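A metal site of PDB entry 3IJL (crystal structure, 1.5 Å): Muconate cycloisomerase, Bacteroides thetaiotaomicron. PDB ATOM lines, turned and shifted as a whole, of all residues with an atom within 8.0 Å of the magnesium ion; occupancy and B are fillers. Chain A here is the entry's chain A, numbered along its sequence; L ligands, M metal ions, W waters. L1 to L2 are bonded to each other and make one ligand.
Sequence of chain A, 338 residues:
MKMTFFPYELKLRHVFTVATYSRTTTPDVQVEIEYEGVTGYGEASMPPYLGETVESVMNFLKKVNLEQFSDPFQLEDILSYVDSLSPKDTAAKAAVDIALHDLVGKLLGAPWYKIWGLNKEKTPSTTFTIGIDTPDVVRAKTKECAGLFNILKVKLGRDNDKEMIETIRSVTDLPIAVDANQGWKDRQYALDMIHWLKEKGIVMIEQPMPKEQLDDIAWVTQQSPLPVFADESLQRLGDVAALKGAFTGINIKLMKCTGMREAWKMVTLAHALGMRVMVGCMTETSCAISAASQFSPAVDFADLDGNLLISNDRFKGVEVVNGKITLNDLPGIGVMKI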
ATOM      1  N   VAL A  18      -2.143 -30.809  -1.858  1.00  0.00           N
ATOM      2  CA  VAL A  18      -2.487 -29.988  -0.713  1.00  0.00           C
ATOM      3  C   VAL A  18      -1.204 -29.892   0.104  1.00  0.00           C
ATOM      4  O   VAL A  18      -0.722 -30.886   0.646  1.00  0.00           O
ATOM      5  CB  VAL A  18      -3.588 -30.638   0.157  1.00  0.00           C
ATOM      6  CG1 VAL A  18      -3.940 -29.727   1.320  1.00  0.00           C
ATOM      7  CG2 VAL A  18      -4.812 -30.919  -0.697  1.00  0.00           C
ATOM      8  N   LYS A 153      -9.274 -19.480  -6.998  1.00  0.00           N
ATOM      9  CA  LYS A 153      -8.602 -19.785  -5.748  1.00  0.00           C
ATOM     10  C   LYS A 153      -7.146 -20.156  -6.015  1.00  0.00           C
ATOM     11  O   LYS A 153      -6.846 -20.831  -7.009  1.00  0.00           O
ATOM     12  CB  LYS A 153      -9.295 -20.945  -5.044  1.00  0.00           C
ATOM     13  CG  LYS A 153      -8.549 -21.480  -3.826  1.00  0.00           C
ATOM     14  CD  LYS A 153      -9.352 -22.601  -3.182  1.00  0.00           C
ATOM     15  CE  LYS A 153      -8.629 -23.227  -2.012  1.00  0.00           C
ATOM     16  NZ  LYS A 153      -9.470 -24.267  -1.359  1.00  0.00           N
ATOM     17  N   LYS A 155      -3.599 -21.471  -3.783  1.00  0.00           N
ATOM     18  CA  LYS A 155      -3.050 -21.916  -2.511  1.00  0.00           C
ATOM     19  C   LYS A 155      -1.650 -21.355  -2.359  1.00  0.00           C
ATOM     20  O   LYS A 155      -0.728 -21.729  -3.089  1.00  0.00           O
ATOM     21  CB  LYS A 155      -3.043 -23.445  -2.455  1.00  0.00           C
ATOM     22  CG  LYS A 155      -4.449 -24.035  -2.318  1.00  0.00           C
ATOM     23  CD  LYS A 155      -4.479 -25.551  -2.450  1.00  0.00           C
ATOM     24  CE  LYS A 155      -4.165 -25.989  -3.867  1.00  0.00           C
ATOM     25  NZ  LYS A 155      -4.472 -27.433  -4.080  1.00  0.00           N
ATOM     26  N   VAL A 178      -7.364 -16.406  -1.638  1.00  0.00           N
ATOM     27  CA  VAL A 178      -6.171 -17.172  -1.332  1.00  0.00           C
ATOM     28  C   VAL A 178      -6.272 -17.967  -0.042  1.00  0.00           C
ATOM     29  O   VAL A 178      -6.892 -17.531   0.933  1.00  0.00           O
ATOM     30  CB  VAL A 178      -4.934 -16.261  -1.226  1.00  0.00           C
ATOM     31  CG1 VAL A 178      -4.714 -15.517  -2.540  1.00  0.00           C
ATOM     32  CG2 VAL A 178      -5.103 -15.281  -0.090  1.00  0.00           C
ATOM     33  N   ASP A 179      -5.662 -19.145  -0.043  1.00  0.00           N
ATOM     34  CA  ASP A 179      -5.637 -19.992   1.141  1.00  0.00           C
ATOM     35  C   ASP A 179      -4.161 -20.220   1.426  1.00  0.00           C
ATOM     36  O   ASP A 179      -3.466 -20.897   0.657  1.00  0.00           O
ATOM     37  CB  ASP A 179      -6.334 -21.337   0.876  1.00  0.00           C
ATOM     38  CG  ASP A 179      -6.519 -22.140   2.151  1.00  0.00           C
ATOM     39  OD1 ASP A 179      -5.801 -21.867   3.126  1.00  0.00           O
ATOM     40  OD2 ASP A 179      -7.376 -23.049   2.166  1.00  0.00           O
ATOM     41  N   ALA A 180      -3.674 -19.636   2.519  1.00  0.00           N
ATOM     42  CA  ALA A 180      -2.266 -19.763   2.900  1.00  0.00           C
ATOM     43  C   ALA A 180      -1.963 -21.066   3.634  1.00  0.00           C
ATOM     44  O   ALA A 180      -0.796 -21.442   3.794  1.00  0.00           O
ATOM     45  CB  ALA A 180      -1.861 -18.575   3.751  1.00  0.00           C
ATOM     46  N   ASN A 181      -3.015 -21.760   4.067  1.00  0.00           N
ATOM     47  CA  ASN A 181      -2.855 -23.020   4.784  1.00  0.00           C
ATOM     48  C   ASN A 181      -1.810 -22.975   5.896  1.00  0.00           C
ATOM     49  O   ASN A 181      -0.906 -23.811   5.950  1.00  0.00           O
ATOM     50  CB  ASN A 181      -2.500 -24.142   3.798  1.00  0.00           C
ATOM     51  CG  ASN A 181      -3.667 -24.544   2.931  1.00  0.00           C
ATOM     52  OD1 ASN A 181      -4.652 -25.109   3.427  1.00  0.00           O
ATOM     53  ND2 ASN A 181      -3.585 -24.261   1.642  1.00  0.00           N
ATOM     54  N   GLN A 182      -1.929 -21.989   6.783  1.00  0.00           N
ATOM     55  CA  GLN A 182      -1.013 -21.838   7.909  1.00  0.00           C
ATOM     56  C   GLN A 182       0.433 -21.660   7.445  1.00  0.00           C
ATOM     57  O   GLN A 182       1.364 -21.928   8.203  1.00  0.00           O
ATOM     58  CB  GLN A 182      -1.094 -23.068   8.816  1.00  0.00           C
ATOM     59  CG  GLN A 182      -2.481 -23.374   9.350  1.00  0.00           C
ATOM     60  CD  GLN A 182      -2.502 -24.613  10.226  1.00  0.00           C
ATOM     61  OE1 GLN A 182      -2.381 -25.740   9.735  1.00  0.00           O
ATOM     62  NE2 GLN A 182      -2.632 -24.413  11.525  1.00  0.00           N
ATOM     63  N   GLU A 206      -7.486 -16.779   3.642  1.00  0.00           N
ATOM     64  CA  GLU A 206      -7.879 -17.923   4.452  1.00  0.00           C
ATOM     65  C   GLU A 206      -6.694 -18.506   5.223  1.00  0.00           C
ATOM     66  O   GLU A 206      -5.620 -18.741   4.656  1.00  0.00           O
ATOM     67  CB  GLU A 206      -8.508 -18.992   3.542  1.00  0.00           C
ATOM     68  CG  GLU A 206      -8.961 -20.255   4.235  1.00  0.00           C
ATOM     69  CD  GLU A 206      -9.609 -21.242   3.272  1.00  0.00           C
ATOM     70  OE1 GLU A 206      -9.862 -22.393   3.699  1.00  0.00           O
ATOM     71  OE2 GLU A 206      -9.860 -20.876   2.104  1.00  0.00           O
ATOM     72  N   GLN A 207      -6.900 -18.706   6.533  1.00  0.00           N
ATOM     73  CA  GLN A 207      -5.886 -19.279   7.441  1.00  0.00           C
ATOM     74  C   GLN A 207      -4.461 -18.833   7.114  1.00  0.00           C
ATOM     75  O   GLN A 207      -3.625 -19.630   6.696  1.00  0.00           O
ATOM     76  CB  GLN A 207      -5.968 -20.813   7.382  1.00  0.00           C
ATOM     77  CG  GLN A 207      -5.306 -21.527   8.557  1.00  0.00           C
ATOM     78  CD  GLN A 207      -6.041 -21.321   9.864  1.00  0.00           C
ATOM     79  OE1 GLN A 207      -7.267 -21.421   9.926  1.00  0.00           O
ATOM     80  NE2 GLN A 207      -5.299 -21.037  10.929  1.00  0.00           N
ATOM     81  N   PHE A 229     -10.476 -15.612   6.960  1.00  0.00           N
ATOM     82  CA  PHE A 229     -11.279 -16.759   7.351  1.00  0.00           C
ATOM     83  C   PHE A 229     -10.493 -17.884   7.993  1.00  0.00           C
ATOM     84  O   PHE A 229      -9.382 -18.193   7.577  1.00  0.00           O
ATOM     85  CB  PHE A 229     -12.035 -17.298   6.134  1.00  0.00           C
ATOM     86  CG  PHE A 229     -13.203 -16.448   5.715  1.00  0.00           C
ATOM     87  CD1 PHE A 229     -14.491 -16.777   6.116  1.00  0.00           C
ATOM     88  CD2 PHE A 229     -13.003 -15.327   4.921  1.00  0.00           C
ATOM     89  CE1 PHE A 229     -15.574 -15.990   5.735  1.00  0.00           C
ATOM     90  CE2 PHE A 229     -14.082 -14.528   4.535  1.00  0.00           C
ATOM     91  CZ  PHE A 229     -15.374 -14.860   4.943  1.00  0.00           C
ATOM     92  N   ALA A 230     -11.102 -18.510   8.996  1.00  0.00           N
ATOM     93  CA  ALA A 230     -10.489 -19.634   9.708  1.00  0.00           C
ATOM     94  C   ALA A 230     -10.890 -20.954   9.076  1.00  0.00           C
ATOM     95  O   ALA A 230     -12.040 -21.148   8.697  1.00  0.00           O
ATOM     96  CB  ALA A 230     -10.911 -19.611  11.173  1.00  0.00           C
ATOM     97  N   ASP A 231      -9.937 -21.878   8.967  1.00  0.00           N
ATOM     98  CA  ASP A 231     -10.194 -23.196   8.406  1.00  0.00           C
ATOM     99  C   ASP A 231      -9.583 -24.222   9.348  1.00  0.00           C
ATOM    100  O   ASP A 231     -10.284 -24.826  10.161  1.00  0.00           O
ATOM    101  CB  ASP A 231      -9.597 -23.324   7.013  1.00  0.00           C
ATOM    102  CG  ASP A 231      -9.970 -24.634   6.328  1.00  0.00           C
ATOM    103  OD1 ASP A 231     -10.538 -25.513   7.003  1.00  0.00           O
ATOM    104  OD2 ASP A 231      -9.688 -24.777   5.125  1.00  0.00           O
ATOM    105  N   GLU A 232      -8.264 -24.400   9.270  1.00  0.00           N
ATOM    106  CA  GLU A 232      -7.593 -25.356  10.140  1.00  0.00           C
ATOM    107  C   GLU A 232      -7.787 -24.996  11.608  1.00  0.00           C
ATOM    108  O   GLU A 232      -7.629 -25.857  12.487  1.00  0.00           O
ATOM    109  CB  GLU A 232      -6.090 -25.411   9.826  1.00  0.00           C
ATOM    110  CG  GLU A 232      -5.724 -26.163   8.550  1.00  0.00           C
ATOM    111  CD  GLU A 232      -6.305 -25.546   7.300  1.00  0.00           C
ATOM    112  OE1 GLU A 232      -6.227 -24.307   7.171  1.00  0.00           O
ATOM    113  OE2 GLU A 232      -6.837 -26.292   6.447  1.00  0.00           O
ATOM    114  N   ASN A 251     -14.730 -21.092   8.054  1.00  0.00           N
ATOM    115  CA  ASN A 251     -14.939 -21.950   6.894  1.00  0.00           C
ATOM    116  C   ASN A 251     -15.564 -23.238   7.431  1.00  0.00           C
ATOM    117  O   ASN A 251     -15.053 -23.836   8.382  1.00  0.00           O
ATOM    118  CB  ASN A 251     -13.607 -22.269   6.201  1.00  0.00           C
ATOM    119  CG  ASN A 251     -13.804 -22.994   4.880  1.00  0.00           C
ATOM    120  OD1 ASN A 251     -14.919 -23.335   4.501  1.00  0.00           O
ATOM    121  ND2 ASN A 251     -12.706 -23.226   4.158  1.00  0.00           N
ATOM    122  N   LYS A 253     -16.926 -27.166   6.595  1.00  0.00           N
ATOM    123  CA  LYS A 253     -16.837 -28.295   5.661  1.00  0.00           C
ATOM    124  C   LYS A 253     -17.585 -29.464   6.294  1.00  0.00           C
ATOM    125  O   LYS A 253     -17.347 -29.805   7.452  1.00  0.00           O
ATOM    126  CB  LYS A 253     -15.389 -28.675   5.386  1.00  0.00           C
ATOM    127  CG  LYS A 253     -14.566 -27.549   4.792  1.00  0.00           C
ATOM    128  CD  LYS A 253     -13.127 -27.989   4.538  1.00  0.00           C
ATOM    129  CE  LYS A 253     -12.214 -26.786   4.388  1.00  0.00           C
ATOM    130  NZ  LYS A 253     -10.780 -27.172   4.248  1.00  0.00           N
ATOM    131  N   LYS A 256     -15.730 -32.198   8.100  1.00  0.00           N
ATOM    132  CA  LYS A 256     -15.088 -31.791   9.348  1.00  0.00           C
ATOM    133  C   LYS A 256     -16.067 -31.588  10.490  1.00  0.00           C
ATOM    134  O   LYS A 256     -15.755 -31.875  11.651  1.00  0.00           O
ATOM    135  CB  LYS A 256     -14.315 -30.479   9.147  1.00  0.00           C
ATOM    136  CG  LYS A 256     -13.135 -30.557   8.179  1.00  0.00           C
ATOM    137  CD  LYS A 256     -12.463 -29.197   8.012  1.00  0.00           C
ATOM    138  CE  LYS A 256     -11.866 -28.674   9.315  1.00  0.00           C
ATOM    139  NZ  LYS A 256     -11.120 -27.401   9.132  1.00  0.00           N
ATOM    140  N   MET A 278     -17.953 -18.983   5.181  1.00  0.00           N
ATOM    141  CA  MET A 278     -17.610 -19.488   3.864  1.00  0.00           C
ATOM    142  C   MET A 278     -17.762 -20.996   3.994  1.00  0.00           C
ATOM    143  O   MET A 278     -17.764 -21.549   5.093  1.00  0.00           O
ATOM    144  CB  MET A 278     -16.175 -19.109   3.458  1.00  0.00           C
ATOM    145  CG  MET A 278     -15.069 -19.869   4.153  1.00  0.00           C
ATOM    146  SD  MET A 278     -13.442 -19.438   3.476  1.00  0.00           S
ATOM    147  CE  MET A 278     -13.434 -20.419   1.969  1.00  0.00           C
ATOM    148  N   GLY A 280     -16.488 -24.872   2.307  1.00  0.00           N
ATOM    149  CA  GLY A 280     -15.522 -25.558   1.472  1.00  0.00           C
ATOM    150  C   GLY A 280     -15.911 -27.003   1.284  1.00  0.00           C
ATOM    151  O   GLY A 280     -17.003 -27.419   1.678  1.00  0.00           O
ATOM    152  N   CYS A 281     -15.016 -27.785   0.711  1.00  0.00           N
ATOM    153  CA  CYS A 281     -15.295 -29.192   0.455  1.00  0.00           C
ATOM    154  C   CYS A 281     -14.017 -29.952   0.157  1.00  0.00           C
ATOM    155  O   CYS A 281     -12.962 -29.362  -0.047  1.00  0.00           O
ATOM    156  CB  CYS A 281     -16.213 -29.336  -0.755  1.00  0.00           C
ATOM    157  SG  CYS A 281     -15.436 -28.816  -2.333  1.00  0.00           S
ATOM    158  N   ASP A 303     -16.151 -22.653  -1.872  1.00  0.00           N
ATOM    159  CA  ASP A 303     -15.224 -23.460  -2.668  1.00  0.00           C
ATOM    160  C   ASP A 303     -16.010 -24.765  -2.726  1.00  0.00           C
ATOM    161  O   ASP A 303     -15.832 -25.652  -1.893  1.00  0.00           O
ATOM    162  CB  ASP A 303     -13.882 -23.651  -1.936  1.00  0.00           C
ATOM    163  CG  ASP A 303     -12.813 -24.246  -2.836  1.00  0.00           C
ATOM    164  OD1 ASP A 303     -12.644 -23.749  -3.970  1.00  0.00           O
ATOM    165  OD2 ASP A 303     -12.126 -25.199  -2.417  1.00  0.00           O
HETATM  166  N1  LIG L   1     -11.533 -27.580  -4.314  1.00  0.00           N
HETATM  167  C1  LIG L   1     -11.709 -28.223  -3.010  1.00  0.00           C
HETATM  168  C2  LIG L   1     -10.398 -27.967  -2.224  1.00  0.00           C
HETATM  169  O1  LIG L   1      -9.477 -27.308  -2.721  1.00  0.00           O
HETATM  170  C3  LIG L   1     -11.912 -29.696  -3.369  1.00  0.00           C
HETATM  171  C4  LIG L   1     -11.050 -29.873  -4.628  1.00  0.00           C
HETATM  172  C5  LIG L   1     -11.241 -28.559  -5.379  1.00  0.00           C
HETATM  173  N1  LG2 L   2     -10.337 -28.490  -0.993  1.00  0.00           N
HETATM  174  C1  LG2 L   2      -9.094 -28.419  -0.171  1.00  0.00           C
HETATM  175  C2  LG2 L   2      -9.353 -27.842   1.221  1.00  0.00           C
HETATM  176  O1  LG2 L   2      -8.390 -27.798   2.030  1.00  0.00           O
HETATM  177  C3  LG2 L   2      -8.464 -29.831  -0.080  1.00  0.00           C
HETATM  178  C4  LG2 L   2      -9.377 -30.971   0.397  1.00  0.00           C
HETATM  179  C5  LG2 L   2      -8.976 -32.312  -0.148  1.00  0.00           C
HETATM  180  O2  LG2 L   2      -7.856 -32.788   0.141  1.00  0.00           O
HETATM  181  O3  LG2 L   2      -9.784 -32.908  -0.885  1.00  0.00           O
HETATM  182  O4  LG2 L   2     -10.493 -27.414   1.508  1.00  0.00           O
HETATM  183 MG    MG M   1      -8.559 -23.884   3.696  1.00  0.00          MG
HETATM  184  O   HOH W   1      -7.174 -23.191   4.992  1.00  0.00           O
HETATM  185  O   HOH W   2      -9.758 -24.739   2.189  1.00  0.00           O
HETATM  186  O   HOH W   3      -7.469 -25.735   3.605  1.00  0.00           O
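The side-chain carboxylate (OD2) of Asp 303 is in salt-bridge range of a nitrogen (N1) of LIG L1 (3.1 Å). The side-chain amino group (NZ) of Lys 253 lies within salt-bridge range of an oxygen (O4) of LG2 L2 (2.8 Å). The backbone carbonyl oxygen of Cys 281 sits at hydrogen-bond distance from a nitrogen (N1) of LG2 L2 (2.9 Å). The side-chain amino group (NZ) of Lys 153 lies within hydrogen-bond range of an oxygen (O1) of LIG L1 (3.3 Å).
The side-chain carboxylate (OE1) of Glu 206 lies close to the side-chain amide nitrogen (ND2) of Asn 251, at 3.0 Å. The backbone NH of Asp 231 is in hydrogen-bond range of the side-chain amide oxygen of Gln 207 (2.9 Å). OD1 of Asp 231 lies within salt-bridge range of NZ of Lys 253 (3.2 Å). The backbone NH (N) of Glu 206 lies within hydrogen-bond range of the backbone carbonyl oxygen (O) of Val 178, 2.9 Å away. N of Asn 181 is in hydrogen-bond range of OD1 of Asp 179, at 2.9 Å. The backbone carbonyl oxygen (O) of Glu 206 sits at hydrogen-bond distance from the backbone NH (N) of Ala 180 (3.0 Å). OD1 of Asp 231 lies within salt-bridge range of NZ of Lys 256, 2.9 Å away.
Of the 21 residues printed, 3 come within 4 Å of the magnesium ion. Along chain A the residues within 4 Å of the magnesium ion span positions 179 to 231. The nearest printed residue that does not touch the magnesium ion is Lys 253 (4.01 Å).
The magnesium ion is bound by the side-chain carboxylate of Glu 206, water W1, the side-chain carboxylate of Asp 231, the side-chain carboxylate of Asp 179, water W2 and water W3. The magnesium ion has six donor atoms within binding distance.
Water W3 lies within hydrogen-bond range of an oxygen (O1) of LG2 L2 (2.8 Å), the side-chain amide oxygen of Asn 181 (2.9 Å) and the side-chain carboxylate of Glu 232 (3.0 Å). Water W2 lies within hydrogen-bond range of an oxygen (O4) of LG2 L2 (2.9 Å) and the side-chain amino group of Lys 253 (3.3 Å). Water W1 lies within hydrogen-bond range of OE1 of Glu 232 and OD1 of Asp 179.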
